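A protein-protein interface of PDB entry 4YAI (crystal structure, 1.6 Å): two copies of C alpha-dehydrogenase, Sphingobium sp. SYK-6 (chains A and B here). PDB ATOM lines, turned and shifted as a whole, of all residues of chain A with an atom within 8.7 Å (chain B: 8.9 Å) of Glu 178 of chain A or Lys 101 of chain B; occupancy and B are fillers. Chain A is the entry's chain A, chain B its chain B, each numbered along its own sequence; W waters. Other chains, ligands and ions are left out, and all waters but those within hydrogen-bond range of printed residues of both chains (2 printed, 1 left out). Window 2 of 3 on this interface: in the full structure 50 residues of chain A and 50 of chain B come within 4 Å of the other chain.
Hydrophobic or aromatic side chains of chain B within 4 Å of the printed part of chain A: Phe 100, Tyr 105 and Trp 108. Of the 17 printed residues of chain A, 7 touch a printed residue of chain B. Hydrophobic or aromatic side chains of chain A that line the printed part of chain B: Met 124, Ile 172 and Met 176. Among the printed residues, Asp or Glu carboxylates within 4 Å of a Lys or Arg side-chain nitrogen of the other chain: Glu 178 of chain A with Lys 101 of chain B (2.9 Å).
Among the printed residues, merely in contact across the chains: Met 124 of chain A with Ala 103 of chain B (3.4 Å), Met 124 of chain A with Tyr 105 of chain B (3.5 Å), Ser 175 of chain A with Ser 153 of chain B (3.5 Å), Ile 172 of chain A with Phe 100 of chain B (3.6 Å), Ser 175 of chain A with Phe 100 of chain B (3.6 Å), Arg 131 of chain A with Lys 101 of chain B (3.8 Å) and Met 176 of chain A with Phe 100 of chain B (3.8 Å).
Water W2 lies within hydrogen-bond range of OG of Ser 175 of chain A (2.7 Å), OE2 of Glu 178 of chain A (2.9 Å) and NZ of Lys 101 of chain B (3.3 Å). Water W1 lies within hydrogen-bond range of OG of Ser 153 of chain B (2.9 Å), N of Phe 154 of chain B (3.0 Å) and OD2 of Asp 174 of chain A (3.2 Å).
No position is printed for both chains.
The guanidinium group of Arg 131 of chain A lies within hydrogen-bond range of the side-chain hydroxyl of Ser 175 of chain A. NH2 of Arg 131 of chain A lies close to SD of Met 176 of chain A (3.6 Å). The side-chain carboxylate (OD2) of Asp 179 of chain A lies within salt-bridge range of the guanidinium group (NH1) of Arg 131 of chain A (2.9 Å). The backbone carbonyl oxygen (O) of Met 176 of chain A sits at hydrogen-bond distance from the backbone NH (N) of Ile 181 of chain A (3.0 Å).
The side-chain sulfur of Met 124 of chain A is in hydrogen-bond range of the indole nitrogen of Trp 108 of chain B (3.7 Å). N of Ser 153 of chain B lies within hydrogen-bond range of OD1 of Asp 174 of chain A (2.8 Å). The side-chain carboxylate (OE1) of Glu 178 of chain A is in salt-bridge range of the side-chain amino group (NZ) of Lys 101 of chain B, at 2.9 Å.
Glu 178 of chain A touches just one residue of chain B: Lys 101. Ser 175 of chain A touches two residues of chain B. No residue of chain B comes within 4 Å of Ala 177 of chain A. Printed residues of chain B within 4 Å of Arg 131 of chain A: Lys 101 (3.8 Å). Of the printed residues of chain A, Phe 100 of chain B touches Ile 172 (3.6 Å), Ser 175 (3.6 Å) and Met 176 (3.8 Å). Of the printed residues of chain B, Met 176 of chain A touches Phe 100. Printed residues of chain A within 4 Å of Tyr 105 of chain B: Met 124 (3.5 Å). Of the printed residues of chain B, Met 124 of chain A touches Ala 103, Tyr 105 and Trp 108. Gly 136 of chain A touches none of the printed residues of chain B. Arg 173 of chain A touches none of the printed residues of chain B. The nearest residue of chain A that does not touch Lys 101 of chain B is Ser 175 of chain A (4.2 Å). The nearest printed residue of chain B that does not touch Met 124 of chain A is Thr 104 of chain B (4.1 Å).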
ATOM      1  N   MET A 124       8.095 -19.077  -8.478  1.00  0.00           N
ATOM      2  CA  MET A 124       7.986 -18.786  -9.901  1.00  0.00           C
ATOM      3  C   MET A 124       9.174 -19.341 -10.690  1.00  0.00           C
ATOM      4  O   MET A 124       9.007 -19.830 -11.809  1.00  0.00           O
ATOM      5  CB  MET A 124       7.876 -17.280 -10.125  1.00  0.00           C
ATOM      6  CG  MET A 124       6.628 -16.653  -9.520  1.00  0.00           C
ATOM      7  SD  MET A 124       5.088 -17.298 -10.198  1.00  0.00           S
ATOM      8  CE  MET A 124       5.234 -16.702 -11.869  1.00  0.00           C
ATOM      9  N   THR A 127       9.253 -23.886  -9.555  1.00  0.00           N
ATOM     10  CA  THR A 127       8.209 -24.902  -9.633  1.00  0.00           C
ATOM     11  C   THR A 127       7.839 -25.327 -11.064  1.00  0.00           C
ATOM     12  O   THR A 127       7.380 -26.449 -11.237  1.00  0.00           O
ATOM     13  CB  THR A 127       6.901 -24.492  -8.870  1.00  0.00           C
ATOM     14  OG1 THR A 127       6.308 -23.313  -9.421  1.00  0.00           O
ATOM     15  CG2 THR A 127       7.182 -24.307  -7.397  1.00  0.00           C
ATOM     16  N   PRO A 128       8.063 -24.478 -12.101  1.00  0.00           N
ATOM     17  CA  PRO A 128       7.779 -25.064 -13.419  1.00  0.00           C
ATOM     18  C   PRO A 128       8.617 -26.315 -13.711  1.00  0.00           C
ATOM     19  O   PRO A 128       8.097 -27.297 -14.254  1.00  0.00           O
ATOM     20  CB  PRO A 128       8.119 -23.926 -14.387  1.00  0.00           C
ATOM     21  CG  PRO A 128       7.882 -22.677 -13.591  1.00  0.00           C
ATOM     22  CD  PRO A 128       8.305 -23.023 -12.185  1.00  0.00           C
ATOM     23  N   ARG A 131       7.376 -29.350 -11.676  1.00  0.00           N
ATOM     24  CA  ARG A 131       6.238 -29.986 -12.325  1.00  0.00           C
ATOM     25  C   ARG A 131       6.715 -30.803 -13.529  1.00  0.00           C
ATOM     26  O   ARG A 131       6.317 -31.954 -13.714  1.00  0.00           O
ATOM     27  CB  ARG A 131       5.205 -28.946 -12.774  1.00  0.00           C
ATOM     28  CG  ARG A 131       4.595 -28.086 -11.676  1.00  0.00           C
ATOM     29  CD  ARG A 131       3.580 -27.142 -12.289  1.00  0.00           C
ATOM     30  NE  ARG A 131       3.154 -26.048 -11.424  1.00  0.00           N
ATOM     31  CZ  ARG A 131       2.117 -26.093 -10.593  1.00  0.00           C
ATOM     32  NH1 ARG A 131       1.412 -27.202 -10.461  1.00  0.00           N
ATOM     33  NH2 ARG A 131       1.798 -25.023  -9.889  1.00  0.00           N
ATOM     34  N   GLY A 134       8.264 -34.280 -13.164  1.00  0.00           N
ATOM     35  CA  GLY A 134       7.243 -35.274 -12.904  1.00  0.00           C
ATOM     36  C   GLY A 134       7.548 -36.291 -11.826  1.00  0.00           C
ATOM     37  O   GLY A 134       6.949 -37.360 -11.829  1.00  0.00           O
ATOM     38  N   GLY A 136       7.377 -35.339  -8.561  1.00  0.00           N
ATOM     39  CA  GLY A 136       6.838 -34.705  -7.375  1.00  0.00           C
ATOM     40  C   GLY A 136       7.878 -33.829  -6.717  1.00  0.00           C
ATOM     41  O   GLY A 136       8.887 -33.493  -7.319  1.00  0.00           O
ATOM     42  N   ILE A 172      -1.445 -21.995  -2.461  1.00  0.00           N
ATOM     43  CA  ILE A 172      -0.811 -22.720  -3.561  1.00  0.00           C
ATOM     44  C   ILE A 172      -0.948 -24.236  -3.429  1.00  0.00           C
ATOM     45  O   ILE A 172      -0.644 -24.965  -4.371  1.00  0.00           O
ATOM     46  CB  ILE A 172       0.691 -22.371  -3.708  1.00  0.00           C
ATOM     47  CG1 ILE A 172       1.496 -22.830  -2.486  1.00  0.00           C
ATOM     48  CG2 ILE A 172       0.854 -20.894  -4.011  1.00  0.00           C
ATOM     49  CD1 ILE A 172       3.000 -22.583  -2.634  1.00  0.00           C
ATOM     50  N   ARG A 173      -1.414 -24.719  -2.278  1.00  0.00           N
ATOM     51  CA  ARG A 173      -1.414 -26.156  -2.009  1.00  0.00           C
ATOM     52  C   ARG A 173      -2.105 -26.975  -3.104  1.00  0.00           C
ATOM     53  O   ARG A 173      -1.544 -27.954  -3.608  1.00  0.00           O
ATOM     54  CB  ARG A 173      -2.076 -26.457  -0.656  1.00  0.00           C
ATOM     55  CG  ARG A 173      -1.855 -27.894  -0.183  1.00  0.00           C
ATOM     56  CD  ARG A 173      -2.487 -28.152   1.169  1.00  0.00           C
ATOM     57  NE  ARG A 173      -1.790 -29.222   1.872  1.00  0.00           N
ATOM     58  CZ  ARG A 173      -2.266 -29.891   2.917  1.00  0.00           C
ATOM     59  NH1 ARG A 173      -3.480 -29.628   3.404  1.00  0.00           N
ATOM     60  NH2 ARG A 173      -1.525 -30.846   3.470  1.00  0.00           N
ATOM     61  N   ASP A 174      -3.314 -26.583  -3.496  1.00  0.00           N
ATOM     62  CA  ASP A 174      -4.065 -27.419  -4.430  1.00  0.00           C
ATOM     63  C   ASP A 174      -3.410 -27.414  -5.814  1.00  0.00           C
ATOM     64  O   ASP A 174      -3.412 -28.438  -6.495  1.00  0.00           O
ATOM     65  CB  ASP A 174      -5.540 -26.990  -4.529  1.00  0.00           C
ATOM     66  CG  ASP A 174      -5.729 -25.624  -5.162  1.00  0.00           C
ATOM     67  OD1 ASP A 174      -5.798 -24.629  -4.414  1.00  0.00           O
ATOM     68  OD2 ASP A 174      -5.843 -25.542  -6.403  1.00  0.00           O
ATOM     69  N   SER A 175      -2.835 -26.286  -6.226  1.00  0.00           N
ATOM     70  CA  SER A 175      -2.139 -26.229  -7.520  1.00  0.00           C
ATOM     71  C   SER A 175      -0.915 -27.139  -7.534  1.00  0.00           C
ATOM     72  O   SER A 175      -0.683 -27.886  -8.498  1.00  0.00           O
ATOM     73  CB  SER A 175      -1.704 -24.802  -7.851  1.00  0.00           C
ATOM     74  OG  SER A 175      -1.013 -24.762  -9.095  1.00  0.00           O
ATOM     75  N   MET A 176      -0.122 -27.067  -6.473  1.00  0.00           N
ATOM     76  CA  MET A 176       1.104 -27.853  -6.402  1.00  0.00           C
ATOM     77  C   MET A 176       0.763 -29.339  -6.330  1.00  0.00           C
ATOM     78  O   MET A 176       1.469 -30.184  -6.887  1.00  0.00           O
ATOM     79  CB  MET A 176       1.946 -27.413  -5.204  1.00  0.00           C
ATOM     80  CG  MET A 176       2.434 -25.982  -5.312  1.00  0.00           C
ATOM     81  SD  MET A 176       3.481 -25.738  -6.765  1.00  0.00           S
ATOM     82  CE  MET A 176       3.400 -23.959  -6.911  1.00  0.00           C
ATOM     83  N   ALA A 177      -0.336 -29.658  -5.660  1.00  0.00           N
ATOM     84  CA  ALA A 177      -0.755 -31.050  -5.503  1.00  0.00           C
ATOM     85  C   ALA A 177      -1.066 -31.707  -6.851  1.00  0.00           C
ATOM     86  O   ALA A 177      -0.980 -32.931  -6.975  1.00  0.00           O
ATOM     87  CB  ALA A 177      -1.959 -31.141  -4.586  1.00  0.00           C
ATOM     88  N   GLU A 178      -1.423 -30.903  -7.854  1.00  0.00           N
ATOM     89  CA  GLU A 178      -1.712 -31.422  -9.191  1.00  0.00           C
ATOM     90  C   GLU A 178      -0.526 -32.215  -9.715  1.00  0.00           C
ATOM     91  O   GLU A 178      -0.685 -33.172 -10.467  1.00  0.00           O
ATOM     92  CB  GLU A 178      -2.041 -30.287 -10.173  1.00  0.00           C
ATOM     93  CG  GLU A 178      -3.288 -29.500  -9.837  1.00  0.00           C
ATOM     94  CD  GLU A 178      -3.476 -28.272 -10.721  1.00  0.00           C
ATOM     95  OE1 GLU A 178      -2.737 -28.116 -11.716  1.00  0.00           O
ATOM     96  OE2 GLU A 178      -4.371 -27.461 -10.413  1.00  0.00           O
ATOM     97  N   ASP A 179       0.668 -31.797  -9.301  1.00  0.00           N
ATOM     98  CA  ASP A 179       1.908 -32.400  -9.764  1.00  0.00           C
ATOM     99  C   ASP A 179       2.670 -33.071  -8.630  1.00  0.00           C
ATOM    100  O   ASP A 179       3.891 -33.226  -8.685  1.00  0.00           O
ATOM    101  CB  ASP A 179       2.769 -31.335 -10.447  1.00  0.00           C
ATOM    102  CG  ASP A 179       2.155 -30.856 -11.744  1.00  0.00           C
ATOM    103  OD1 ASP A 179       2.174 -31.637 -12.717  1.00  0.00           O
ATOM    104  OD2 ASP A 179       1.626 -29.724 -11.784  1.00  0.00           O
ATOM    105  N   ASN A 180       1.923 -33.482  -7.605  1.00  0.00           N
ATOM    106  CA  ASN A 180       2.459 -34.235  -6.480  1.00  0.00           C
ATOM    107  C   ASN A 180       3.577 -33.474  -5.783  1.00  0.00           C
ATOM    108  O   ASN A 180       4.541 -34.068  -5.304  1.00  0.00           O
ATOM    109  CB  ASN A 180       2.957 -35.607  -6.941  1.00  0.00           C
ATOM    110  CG  ASN A 180       3.126 -36.589  -5.787  1.00  0.00           C
ATOM    111  OD1 ASN A 180       2.580 -36.392  -4.697  1.00  0.00           O
ATOM    112  ND2 ASN A 180       3.888 -37.652  -6.023  1.00  0.00           N
ATOM    113  N   ILE A 181       3.426 -32.155  -5.739  1.00  0.00           N
ATOM    114  CA  ILE A 181       4.291 -31.286  -4.959  1.00  0.00           C
ATOM    115  C   ILE A 181       3.539 -30.864  -3.705  1.00  0.00           C
ATOM    116  O   ILE A 181       2.504 -30.204  -3.795  1.00  0.00           O
ATOM    117  CB  ILE A 181       4.725 -30.053  -5.767  1.00  0.00           C
ATOM    118  CG1 ILE A 181       5.511 -30.481  -7.006  1.00  0.00           C
ATOM    119  CG2 ILE A 181       5.563 -29.095  -4.915  1.00  0.00           C
ATOM    120  CD1 ILE A 181       5.630 -29.405  -8.053  1.00  0.00           C
ATOM    121  N   GLY A 182       4.045 -31.260  -2.542  1.00  0.00           N
ATOM    122  CA  GLY A 182       3.450 -30.859  -1.276  1.00  0.00           C
ATOM    123  C   GLY A 182       4.017 -29.544  -0.790  1.00  0.00           C
ATOM    124  O   GLY A 182       5.084 -29.117  -1.255  1.00  0.00           O
ATOM    125  N   GLY B  98      -6.995 -16.031 -11.338  1.00  0.00           N
ATOM    126  CA  GLY B  98      -6.897 -16.803 -12.560  1.00  0.00           C
ATOM    127  C   GLY B  98      -6.142 -18.089 -12.288  1.00  0.00           C
ATOM    128  O   GLY B  98      -5.600 -18.260 -11.193  1.00  0.00           O
ATOM    129  N   PRO B  99      -6.095 -18.993 -13.274  1.00  0.00           N
ATOM    130  CA  PRO B  99      -5.359 -20.253 -13.127  1.00  0.00           C
ATOM    131  C   PRO B  99      -3.942 -19.983 -12.643  1.00  0.00           C
ATOM    132  O   PRO B  99      -3.228 -19.187 -13.251  1.00  0.00           O
ATOM    133  CB  PRO B  99      -5.378 -20.837 -14.537  1.00  0.00           C
ATOM    134  CG  PRO B  99      -6.593 -20.246 -15.167  1.00  0.00           C
ATOM    135  CD  PRO B  99      -6.694 -18.859 -14.610  1.00  0.00           C
ATOM    136  N   PHE B 100      -3.551 -20.605 -11.534  1.00  0.00           N
ATOM    137  CA  PHE B 100      -2.295 -20.251 -10.887  1.00  0.00           C
ATOM    138  C   PHE B 100      -1.087 -20.442 -11.809  1.00  0.00           C
ATOM    139  O   PHE B 100      -0.160 -19.634 -11.784  1.00  0.00           O
ATOM    140  CB  PHE B 100      -2.102 -21.068  -9.608  1.00  0.00           C
ATOM    141  CG  PHE B 100      -0.869 -20.685  -8.838  1.00  0.00           C
ATOM    142  CD1 PHE B 100      -0.883 -19.604  -7.985  1.00  0.00           C
ATOM    143  CD2 PHE B 100       0.308 -21.388  -9.000  1.00  0.00           C
ATOM    144  CE1 PHE B 100       0.251 -19.240  -7.289  1.00  0.00           C
ATOM    145  CE2 PHE B 100       1.447 -21.024  -8.307  1.00  0.00           C
ATOM    146  CZ  PHE B 100       1.420 -19.955  -7.462  1.00  0.00           C
ATOM    147  N   LYS B 101      -1.101 -21.491 -12.626  1.00  0.00           N
ATOM    148  CA  LYS B 101       0.026 -21.758 -13.517  1.00  0.00           C
ATOM    149  C   LYS B 101       0.153 -20.707 -14.622  1.00  0.00           C
ATOM    150  O   LYS B 101       1.222 -20.550 -15.212  1.00  0.00           O
ATOM    151  CB  LYS B 101      -0.102 -23.151 -14.131  1.00  0.00           C
ATOM    152  CG  LYS B 101      -0.025 -24.271 -13.107  1.00  0.00           C
ATOM    153  CD  LYS B 101       0.122 -25.635 -13.765  1.00  0.00           C
ATOM    154  CE  LYS B 101      -1.092 -26.002 -14.602  1.00  0.00           C
ATOM    155  NZ  LYS B 101      -2.319 -26.095 -13.778  1.00  0.00           N
ATOM    156  N   ASP B 102      -0.925 -19.975 -14.890  1.00  0.00           N
ATOM    157  CA  ASP B 102      -0.915 -18.957 -15.941  1.00  0.00           C
ATOM    158  C   ASP B 102      -0.382 -17.613 -15.450  1.00  0.00           C
ATOM    159  O   ASP B 102       0.073 -16.797 -16.249  1.00  0.00           O
ATOM    160  CB  ASP B 102      -2.319 -18.764 -16.518  1.00  0.00           C
ATOM    161  CG  ASP B 102      -2.818 -19.982 -17.297  1.00  0.00           C
ATOM    162  OD1 ASP B 102      -2.043 -20.935 -17.516  1.00  0.00           O
ATOM    163  OD2 ASP B 102      -3.998 -19.971 -17.686  1.00  0.00           O
ATOM    164  N   ALA B 103      -0.431 -17.384 -14.140  1.00  0.00           N
ATOM    165  CA  ALA B 103       0.000 -16.114 -13.560  1.00  0.00           C
ATOM    166  C   ALA B 103       1.490 -15.862 -13.802  1.00  0.00           C
ATOM    167  O   ALA B 103       2.315 -16.775 -13.677  1.00  0.00           O
ATOM    168  CB  ALA B 103      -0.305 -16.090 -12.072  1.00  0.00           C
ATOM    169  N   THR B 104       1.824 -14.628 -14.175  1.00  0.00           N
ATOM    170  CA  THR B 104       3.208 -14.239 -14.442  1.00  0.00           C
ATOM    171  C   THR B 104       3.670 -13.261 -13.378  1.00  0.00           C
ATOM    172  O   THR B 104       2.880 -12.855 -12.529  1.00  0.00           O
ATOM    173  CB  THR B 104       3.361 -13.579 -15.814  1.00  0.00           C
ATOM    174  OG1 THR B 104       2.622 -12.352 -15.838  1.00  0.00           O
ATOM    175  CG2 THR B 104       2.850 -14.505 -16.909  1.00  0.00           C
ATOM    176  N   TYR B 105       4.943 -12.876 -13.416  1.00  0.00           N
ATOM    177  CA  TYR B 105       5.430 -11.863 -12.482  1.00  0.00           C
ATOM    178  C   TYR B 105       4.620 -10.566 -12.585  1.00  0.00           C
ATOM    179  O   TYR B 105       4.377  -9.891 -11.590  1.00  0.00           O
ATOM    180  CB  TYR B 105       6.900 -11.558 -12.730  1.00  0.00           C
ATOM    181  CG  TYR B 105       7.880 -12.515 -12.084  1.00  0.00           C
ATOM    182  CD1 TYR B 105       7.797 -12.832 -10.738  1.00  0.00           C
ATOM    183  CD2 TYR B 105       8.905 -13.081 -12.821  1.00  0.00           C
ATOM    184  CE1 TYR B 105       8.701 -13.702 -10.147  1.00  0.00           C
ATOM    185  CE2 TYR B 105       9.813 -13.949 -12.237  1.00  0.00           C
ATOM    186  CZ  TYR B 105       9.712 -14.244 -10.901  1.00  0.00           C
ATOM    187  OH  TYR B 105      10.632 -15.098 -10.330  1.00  0.00           O
ATOM    188  N   ASP B 107       1.491 -10.284 -13.121  1.00  0.00           N
ATOM    189  CA  ASP B 107       0.259 -10.473 -12.360  1.00  0.00           C
ATOM    190  C   ASP B 107       0.494 -10.394 -10.847  1.00  0.00           C
ATOM    191  O   ASP B 107      -0.287  -9.783 -10.116  1.00  0.00           O
ATOM    192  CB  ASP B 107      -0.382 -11.800 -12.749  1.00  0.00           C
ATOM    193  CG  ASP B 107      -0.744 -11.842 -14.226  1.00  0.00           C
ATOM    194  OD1 ASP B 107      -1.334 -10.855 -14.722  1.00  0.00           O
ATOM    195  OD2 ASP B 107      -0.411 -12.836 -14.902  1.00  0.00           O
ATOM    196  N   TRP B 108       1.579 -10.990 -10.371  1.00  0.00           N
ATOM    197  CA  TRP B 108       1.947 -10.847  -8.965  1.00  0.00           C
ATOM    198  C   TRP B 108       2.213  -9.385  -8.608  1.00  0.00           C
ATOM    199  O   TRP B 108       1.722  -8.884  -7.597  1.00  0.00           O
ATOM    200  CB  TRP B 108       3.182 -11.683  -8.641  1.00  0.00           C
ATOM    201  CG  TRP B 108       2.868 -13.083  -8.223  1.00  0.00           C
ATOM    202  CD1 TRP B 108       3.098 -14.222  -8.930  1.00  0.00           C
ATOM    203  CD2 TRP B 108       2.265 -13.484  -6.992  1.00  0.00           C
ATOM    204  NE1 TRP B 108       2.669 -15.318  -8.210  1.00  0.00           N
ATOM    205  CE2 TRP B 108       2.162 -14.886  -7.014  1.00  0.00           C
ATOM    206  CE3 TRP B 108       1.812 -12.791  -5.868  1.00  0.00           C
ATOM    207  CZ2 TRP B 108       1.607 -15.608  -5.949  1.00  0.00           C
ATOM    208  CZ3 TRP B 108       1.266 -13.509  -4.823  1.00  0.00           C
ATOM    209  CH2 TRP B 108       1.167 -14.895  -4.875  1.00  0.00           C
ATOM    210  N   SER B 153      -6.002 -21.975  -5.105  1.00  0.00           N
ATOM    211  CA  SER B 153      -4.866 -21.391  -5.803  1.00  0.00           C
ATOM    212  C   SER B 153      -5.266 -20.365  -6.862  1.00  0.00           C
ATOM    213  O   SER B 153      -4.494 -19.467  -7.170  1.00  0.00           O
ATOM    214  CB  SER B 153      -4.045 -22.507  -6.460  1.00  0.00           C
ATOM    215  OG  SER B 153      -4.812 -23.177  -7.446  1.00  0.00           O
ATOM    216  N   PHE B 154      -6.456 -20.531  -7.433  1.00  0.00           N
ATOM    217  CA  PHE B 154      -7.028 -19.588  -8.390  1.00  0.00           C
ATOM    218  C   PHE B 154      -7.041 -18.154  -7.828  1.00  0.00           C
ATOM    219  O   PHE B 154      -6.978 -17.186  -8.582  1.00  0.00           O
ATOM    220  CB  PHE B 154      -8.455 -20.058  -8.750  1.00  0.00           C
ATOM    221  CG  PHE B 154      -9.099 -19.302  -9.877  1.00  0.00           C
ATOM    222  CD1 PHE B 154      -9.802 -18.136  -9.632  1.00  0.00           C
ATOM    223  CD2 PHE B 154      -9.033 -19.779 -11.175  1.00  0.00           C
ATOM    224  CE1 PHE B 154     -10.415 -17.445 -10.670  1.00  0.00           C
ATOM    225  CE2 PHE B 154      -9.646 -19.091 -12.221  1.00  0.00           C
ATOM    226  CZ  PHE B 154     -10.333 -17.924 -11.964  1.00  0.00           C
ATOM    227  N   ALA B 156      -4.811 -17.053  -5.328  1.00  0.00           N
ATOM    228  CA  ALA B 156      -3.593 -16.927  -4.526  1.00  0.00           C
ATOM    229  C   ALA B 156      -3.131 -15.470  -4.366  1.00  0.00           C
ATOM    230  O   ALA B 156      -2.811 -15.035  -3.253  1.00  0.00           O
ATOM    231  CB  ALA B 156      -2.475 -17.763  -5.134  1.00  0.00           C
ATOM    232  N   GLY B 211      -0.525 -13.012 -17.824  1.00  0.00           N
ATOM    233  CA  GLY B 211      -0.967 -14.321 -18.267  1.00  0.00           C
ATOM    234  C   GLY B 211      -2.454 -14.551 -18.073  1.00  0.00           C
ATOM    235  O   GLY B 211      -2.953 -15.636 -18.377  1.00  0.00           O
ATOM    236  N   LEU B 212      -3.160 -13.531 -17.589  1.00  0.00           N
ATOM    237  CA  LEU B 212      -4.532 -13.699 -17.113  1.00  0.00           C
ATOM    238  C   LEU B 212      -5.573 -12.856 -17.848  1.00  0.00           C
ATOM    239  O   LEU B 212      -6.666 -12.638 -17.325  1.00  0.00           O
ATOM    240  CB  LEU B 212      -4.598 -13.363 -15.623  1.00  0.00           C
ATOM    241  CG  LEU B 212      -3.680 -14.207 -14.737  1.00  0.00           C
ATOM    242  CD1 LEU B 212      -3.802 -13.767 -13.281  1.00  0.00           C
ATOM    243  CD2 LEU B 212      -3.987 -15.693 -14.888  1.00  0.00           C
HETATM  244  O   HOH W   1      -7.717 -23.281  -7.678  1.00  0.00           O
HETATM  245  O   HOH W   2      -3.128 -24.891 -10.828  1.00  0.00           O
